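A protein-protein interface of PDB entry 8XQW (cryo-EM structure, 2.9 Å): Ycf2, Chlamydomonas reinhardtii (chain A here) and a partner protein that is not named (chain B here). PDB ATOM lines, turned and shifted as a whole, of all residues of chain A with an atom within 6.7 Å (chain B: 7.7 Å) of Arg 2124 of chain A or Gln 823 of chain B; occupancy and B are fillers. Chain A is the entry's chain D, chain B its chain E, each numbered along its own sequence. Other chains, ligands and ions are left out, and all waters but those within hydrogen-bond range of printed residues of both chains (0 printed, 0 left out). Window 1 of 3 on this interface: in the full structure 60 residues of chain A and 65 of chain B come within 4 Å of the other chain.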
ATOM      1  N   GLY A2121      14.230  16.900 -18.753  1.00  0.00           N
ATOM      2  CA  GLY A2121      13.977  15.657 -19.445  1.00  0.00           C
ATOM      3  C   GLY A2121      12.641  15.007 -19.171  1.00  0.00           C
ATOM      4  O   GLY A2121      12.518  13.790 -19.352  1.00  0.00           O
ATOM      5  N   SER A2122      11.637  15.769 -18.726  1.00  0.00           N
ATOM      6  CA  SER A2122      10.331  15.217 -18.382  1.00  0.00           C
ATOM      7  C   SER A2122       9.768  14.377 -19.522  1.00  0.00           C
ATOM      8  O   SER A2122       9.575  13.167 -19.371  1.00  0.00           O
ATOM      9  CB  SER A2122       9.355  16.337 -18.025  1.00  0.00           C
ATOM     10  OG  SER A2122       8.773  16.886 -19.191  1.00  0.00           O
ATOM     11  N   GLN A2123       9.516  15.011 -20.664  1.00  0.00           N
ATOM     12  CA  GLN A2123       9.166  14.314 -21.900  1.00  0.00           C
ATOM     13  C   GLN A2123       7.974  13.378 -21.707  1.00  0.00           C
ATOM     14  O   GLN A2123       7.993  12.217 -22.115  1.00  0.00           O
ATOM     15  CB  GLN A2123      10.374  13.552 -22.445  1.00  0.00           C
ATOM     16  CG  GLN A2123      11.654  14.371 -22.468  1.00  0.00           C
ATOM     17  CD  GLN A2123      12.805  13.647 -23.137  1.00  0.00           C
ATOM     18  OE1 GLN A2123      12.612  12.912 -24.102  1.00  0.00           O
ATOM     19  NE2 GLN A2123      14.013  13.858 -22.631  1.00  0.00           N
ATOM     20  N   ARG A2124       6.931  13.883 -21.063  1.00  0.00           N
ATOM     21  CA  ARG A2124       5.705  13.105 -20.898  1.00  0.00           C
ATOM     22  C   ARG A2124       4.639  13.524 -21.900  1.00  0.00           C
ATOM     23  O   ARG A2124       3.582  14.036 -21.542  1.00  0.00           O
ATOM     24  CB  ARG A2124       5.189  13.211 -19.468  1.00  0.00           C
ATOM     25  CG  ARG A2124       5.066  14.617 -18.917  1.00  0.00           C
ATOM     26  CD  ARG A2124       4.683  14.590 -17.442  1.00  0.00           C
ATOM     27  NE  ARG A2124       3.574  13.680 -17.160  1.00  0.00           N
ATOM     28  CZ  ARG A2124       3.695  12.519 -16.518  1.00  0.00           C
ATOM     29  NH1 ARG A2124       2.626  11.763 -16.309  1.00  0.00           N
ATOM     30  NH2 ARG A2124       4.882  12.115 -16.088  1.00  0.00           N
ATOM     31  N   ASP A2125       4.915  13.299 -23.182  1.00  0.00           N
ATOM     32  CA  ASP A2125       3.929  13.511 -24.228  1.00  0.00           C
ATOM     33  C   ASP A2125       4.368  12.762 -25.474  1.00  0.00           C
ATOM     34  O   ASP A2125       5.563  12.641 -25.753  1.00  0.00           O
ATOM     35  CB  ASP A2125       3.743  14.993 -24.541  1.00  0.00           C
ATOM     36  CG  ASP A2125       2.335  15.314 -24.956  1.00  0.00           C
ATOM     37  OD1 ASP A2125       1.580  14.363 -25.238  1.00  0.00           O
ATOM     38  OD2 ASP A2125       1.980  16.509 -25.000  1.00  0.00           O
ATOM     39  N   GLU A2126       3.391  12.260 -26.222  1.00  0.00           N
ATOM     40  CA  GLU A2126       3.716  11.446 -27.378  1.00  0.00           C
ATOM     41  C   GLU A2126       4.232  12.306 -28.521  1.00  0.00           C
ATOM     42  O   GLU A2126       3.924  13.493 -28.632  1.00  0.00           O
ATOM     43  CB  GLU A2126       2.502  10.646 -27.833  1.00  0.00           C
ATOM     44  CG  GLU A2126       2.617   9.179 -27.503  1.00  0.00           C
ATOM     45  CD  GLU A2126       3.935   8.578 -27.965  1.00  0.00           C
ATOM     46  OE1 GLU A2126       4.449   7.674 -27.273  1.00  0.00           O
ATOM     47  OE2 GLU A2126       4.457   8.997 -29.020  1.00  0.00           O
ATOM     48  N   LYS A2130       3.458  16.440 -29.819  1.00  0.00           N
ATOM     49  CA  LYS A2130       4.449  17.502 -29.902  1.00  0.00           C
ATOM     50  C   LYS A2130       4.553  18.046 -31.317  1.00  0.00           C
ATOM     51  O   LYS A2130       4.594  19.266 -31.526  1.00  0.00           O
ATOM     52  CB  LYS A2130       5.798  16.979 -29.427  1.00  0.00           C
ATOM     53  CG  LYS A2130       5.756  16.408 -28.031  1.00  0.00           C
ATOM     54  CD  LYS A2130       6.724  15.261 -27.875  1.00  0.00           C
ATOM     55  CE  LYS A2130       8.136  15.674 -28.213  1.00  0.00           C
ATOM     56  NZ  LYS A2130       9.075  14.522 -28.149  1.00  0.00           N
ATOM     57  N   GLY B 817      13.280  15.309 -12.537  1.00  0.00           N
ATOM     58  CA  GLY B 817      11.982  15.957 -12.763  1.00  0.00           C
ATOM     59  C   GLY B 817      11.316  16.277 -11.450  1.00  0.00           C
ATOM     60  O   GLY B 817      10.148  16.690 -11.461  1.00  0.00           O
ATOM     61  N   VAL B 820      10.906  20.201 -11.074  1.00  0.00           N
ATOM     62  CA  VAL B 820       9.817  20.940 -11.689  1.00  0.00           C
ATOM     63  C   VAL B 820       8.602  20.929 -10.775  1.00  0.00           C
ATOM     64  O   VAL B 820       8.492  20.113  -9.855  1.00  0.00           O
ATOM     65  CB  VAL B 820       9.461  20.341 -13.058  1.00  0.00           C
ATOM     66  CG1 VAL B 820       8.809  21.382 -13.924  1.00  0.00           C
ATOM     67  CG2 VAL B 820      10.686  19.796 -13.727  1.00  0.00           C
ATOM     68  N   ILE B 821       7.674  21.848 -11.031  1.00  0.00           N
ATOM     69  CA  ILE B 821       6.381  21.860 -10.351  1.00  0.00           C
ATOM     70  C   ILE B 821       5.462  20.934 -11.143  1.00  0.00           C
ATOM     71  O   ILE B 821       4.669  21.385 -11.970  1.00  0.00           O
ATOM     72  CB  ILE B 821       5.807  23.274 -10.246  1.00  0.00           C
ATOM     73  CG1 ILE B 821       6.917  24.274  -9.913  1.00  0.00           C
ATOM     74  CG2 ILE B 821       4.705  23.314  -9.205  1.00  0.00           C
ATOM     75  CD1 ILE B 821       7.625  24.005  -8.610  1.00  0.00           C
ATOM     76  N   GLY B 822       5.547  19.634 -10.863  1.00  0.00           N
ATOM     77  CA  GLY B 822       5.042  18.625 -11.772  1.00  0.00           C
ATOM     78  C   GLY B 822       3.528  18.528 -11.847  1.00  0.00           C
ATOM     79  O   GLY B 822       2.787  19.325 -11.278  1.00  0.00           O
ATOM     80  N   GLN B 823       3.080  17.511 -12.583  1.00  0.00           N
ATOM     81  CA  GLN B 823       1.667  17.236 -12.807  1.00  0.00           C
ATOM     82  C   GLN B 823       1.392  15.740 -12.697  1.00  0.00           C
ATOM     83  O   GLN B 823       2.248  14.981 -12.228  1.00  0.00           O
ATOM     84  CB  GLN B 823       1.237  17.753 -14.178  1.00  0.00           C
ATOM     85  CG  GLN B 823       2.075  17.198 -15.317  1.00  0.00           C
ATOM     86  CD  GLN B 823       1.264  16.934 -16.566  1.00  0.00           C
ATOM     87  OE1 GLN B 823       0.363  17.698 -16.910  1.00  0.00           O
ATOM     88  NE2 GLN B 823       1.582  15.849 -17.258  1.00  0.00           N
ATOM     89  N   GLN B 824       0.207  15.305 -13.120  1.00  0.00           N
ATOM     90  CA  GLN B 824      -0.118  13.883 -13.135  1.00  0.00           C
ATOM     91  C   GLN B 824      -1.181  13.622 -14.188  1.00  0.00           C
ATOM     92  O   GLN B 824      -2.213  14.298 -14.210  1.00  0.00           O
ATOM     93  CB  GLN B 824      -0.608  13.410 -11.765  1.00  0.00           C
ATOM     94  CG  GLN B 824      -0.130  12.014 -11.398  1.00  0.00           C
ATOM     95  CD  GLN B 824      -0.549  10.965 -12.410  1.00  0.00           C
ATOM     96  OE1 GLN B 824      -1.710  10.905 -12.814  1.00  0.00           O
ATOM     97  NE2 GLN B 824       0.397  10.134 -12.828  1.00  0.00           N
ATOM     98  N   ARG B 825      -0.933  12.635 -15.047  1.00  0.00           N
ATOM     99  CA  ARG B 825      -1.855  12.262 -16.106  1.00  0.00           C
ATOM    100  C   ARG B 825      -2.002  10.746 -16.169  1.00  0.00           C
ATOM    101  O   ARG B 825      -1.219   9.996 -15.579  1.00  0.00           O
ATOM    102  CB  ARG B 825      -1.393  12.807 -17.464  1.00  0.00           C
ATOM    103  CG  ARG B 825      -1.354  14.325 -17.530  1.00  0.00           C
ATOM    104  CD  ARG B 825      -2.744  14.912 -17.324  1.00  0.00           C
ATOM    105  NE  ARG B 825      -2.776  16.356 -17.528  1.00  0.00           N
ATOM    106  CZ  ARG B 825      -2.686  17.252 -16.549  1.00  0.00           C
ATOM    107  NH1 ARG B 825      -2.556  16.854 -15.293  1.00  0.00           N
ATOM    108  NH2 ARG B 825      -2.726  18.545 -16.824  1.00  0.00           N
ATOM    109  N   ALA B 826      -3.024  10.303 -16.903  1.00  0.00           N
ATOM    110  CA  ALA B 826      -3.350   8.889 -17.047  1.00  0.00           C
ATOM    111  C   ALA B 826      -2.744   8.270 -18.302  1.00  0.00           C
ATOM    112  O   ALA B 826      -3.345   7.362 -18.888  1.00  0.00           O
ATOM    113  CB  ALA B 826      -4.866   8.698 -17.051  1.00  0.00           C
ATOM    114  N   ARG B 827      -1.581   8.746 -18.727  1.00  0.00           N
ATOM    115  CA  ARG B 827      -0.979   8.275 -19.961  1.00  0.00           C
ATOM    116  C   ARG B 827       0.093   7.228 -19.674  1.00  0.00           C
ATOM    117  O   ARG B 827       0.639   7.138 -18.574  1.00  0.00           O
ATOM    118  CB  ARG B 827      -0.376   9.449 -20.726  1.00  0.00           C
ATOM    119  CG  ARG B 827      -1.206  10.714 -20.619  1.00  0.00           C
ATOM    120  CD  ARG B 827      -0.537  11.871 -21.325  1.00  0.00           C
ATOM    121  NE  ARG B 827       0.639  12.334 -20.597  1.00  0.00           N
ATOM    122  CZ  ARG B 827       0.864  13.600 -20.266  1.00  0.00           C
ATOM    123  NH1 ARG B 827      -0.005  14.543 -20.606  1.00  0.00           N
ATOM    124  NH2 ARG B 827       1.963  13.926 -19.605  1.00  0.00           N
ATOM    125  N   LYS B 828       0.392   6.430 -20.694  1.00  0.00           N
ATOM    126  CA  LYS B 828       1.485   5.477 -20.634  1.00  0.00           C
ATOM    127  C   LYS B 828       2.807   6.188 -20.918  1.00  0.00           C
ATOM    128  O   LYS B 828       2.871   7.412 -21.039  1.00  0.00           O
ATOM    129  CB  LYS B 828       1.249   4.343 -21.624  1.00  0.00           C
ATOM    130  CG  LYS B 828       0.810   4.832 -22.977  1.00  0.00           C
ATOM    131  CD  LYS B 828       0.990   3.754 -24.014  1.00  0.00           C
ATOM    132  CE  LYS B 828       2.456   3.435 -24.220  1.00  0.00           C
ATOM    133  NZ  LYS B 828       2.664   2.643 -25.461  1.00  0.00           N
ATOM    134  N   VAL B 829       3.869   5.420 -21.036  1.00  0.00           N
ATOM    135  CA  VAL B 829       5.185   5.984 -21.297  1.00  0.00           C
ATOM    136  C   VAL B 829       5.320   6.245 -22.787  1.00  0.00           C
ATOM    137  O   VAL B 829       4.835   5.473 -23.620  1.00  0.00           O
ATOM    138  CB  VAL B 829       6.300   5.063 -20.775  1.00  0.00           C
ATOM    139  CG1 VAL B 829       6.125   4.832 -19.290  1.00  0.00           C
ATOM    140  CG2 VAL B 829       6.285   3.749 -21.501  1.00  0.00           C
ATOM    141  N   VAL B 830       5.956   7.368 -23.121  1.00  0.00           N
ATOM    142  CA  VAL B 830       6.062   7.792 -24.506  1.00  0.00           C
ATOM    143  C   VAL B 830       6.835   6.750 -25.309  1.00  0.00           C
ATOM    144  O   VAL B 830       7.611   5.955 -24.765  1.00  0.00           O
ATOM    145  CB  VAL B 830       6.727   9.175 -24.563  1.00  0.00           C
ATOM    146  CG1 VAL B 830       6.947   9.652 -25.986  1.00  0.00           C
ATOM    147  CG2 VAL B 830       5.896  10.170 -23.775  1.00  0.00           C
ATOM    148  N   ASP B 833      10.978   8.725 -26.535  1.00  0.00           N
ATOM    149  CA  ASP B 833      11.643   9.832 -25.860  1.00  0.00           C
ATOM    150  C   ASP B 833      11.521   9.747 -24.349  1.00  0.00           C
ATOM    151  O   ASP B 833      12.407  10.222 -23.633  1.00  0.00           O
ATOM    152  CB  ASP B 833      11.102  11.165 -26.375  1.00  0.00           C
ATOM    153  CG  ASP B 833      11.491  11.430 -27.820  1.00  0.00           C
ATOM    154  OD1 ASP B 833      12.264  10.627 -28.384  1.00  0.00           O
ATOM    155  OD2 ASP B 833      11.045  12.450 -28.388  1.00  0.00           O
ATOM    156  N   ALA B 834      10.452   9.146 -23.835  1.00  0.00           N
ATOM    157  CA  ALA B 834      10.400   8.906 -22.401  1.00  0.00           C
ATOM    158  C   ALA B 834      10.911   7.525 -22.037  1.00  0.00           C
ATOM    159  O   ALA B 834      11.260   7.286 -20.877  1.00  0.00           O
ATOM    160  CB  ALA B 834       8.976   9.084 -21.874  1.00  0.00           C
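The side-chain amide oxygen of Gln 2123 of chain A sits close to the backbone carbonyl oxygen of Asp 833 of chain B (2.7 Å).
The backbone carbonyl oxygen (O) of Arg 2124 of chain A is in hydrogen-bond range of the guanidinium group (NH2) of Arg 827 of chain B (2.5 Å).
The side-chain carboxylate (OD2) of Asp 833 of chain B is in salt-bridge range of the side-chain amino group (NZ) of Lys 2130 of chain A (2.9 Å).
The guanidinium group (NE) of Arg 2124 of chain A sits close to the side-chain amide nitrogen (NE2) of Gln 823 of chain B (2.9 Å).
The guanidinium group (NH2) of Arg 825 of chain B lies close to the side-chain amide oxygen (OE1) of Gln 823 of chain B, 3.2 Å away.
The guanidinium group (NH2) of Arg 827 of chain B lies close to the side-chain amide nitrogen (NE2) of Gln 823 of chain B (3.1 Å).
Among the printed residues, merely in contact across the chains: Gln 2123 of chain A with Val 830 of chain B, Gln 2123 of chain A with Ala 834 of chain B, Arg 2124 of chain A with Arg 825 of chain B, Asp 2125 of chain A with Val 830 of chain B and Glu 2126 of chain A with Val 830 of chain B.
Of chain B, only Gln 823, Arg 825 and Arg 827 come within 4 Å of Arg 2124 of chain A.
Gln 823 of chain B touches just one residue of chain A: Arg 2124 (2.9 Å).
Of the printed residues of chain B, Glu 2126 of chain A touches Val 830 (3.2 Å).
Of the printed residues of chain A, Arg 825 of chain B touches Arg 2124.
Of the printed residues of chain B, Asp 2125 of chain A touches Val 830 (3.2 Å).
Of the printed residues of chain A, Ala 834 of chain B touches Gln 2123.
Gly 817 of chain B touches none of the printed residues of chain A.
The nearest residue of chain B that does not touch Arg 2124 of chain A is Val 830 of chain B (4.04 Å).
The nearest printed residue of chain A that does not touch Arg 827 of chain B is Asp 2125 of chain A (4.7 Å).
Along chain A the printed residues that touch a printed residue of chain B span positions 2123 to 2130.
Among the printed residues, Asp or Glu carboxylates within 4 Å of a Lys or Arg side-chain nitrogen of the other chain: Lys 2130 of chain A with Asp 833 of chain B.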
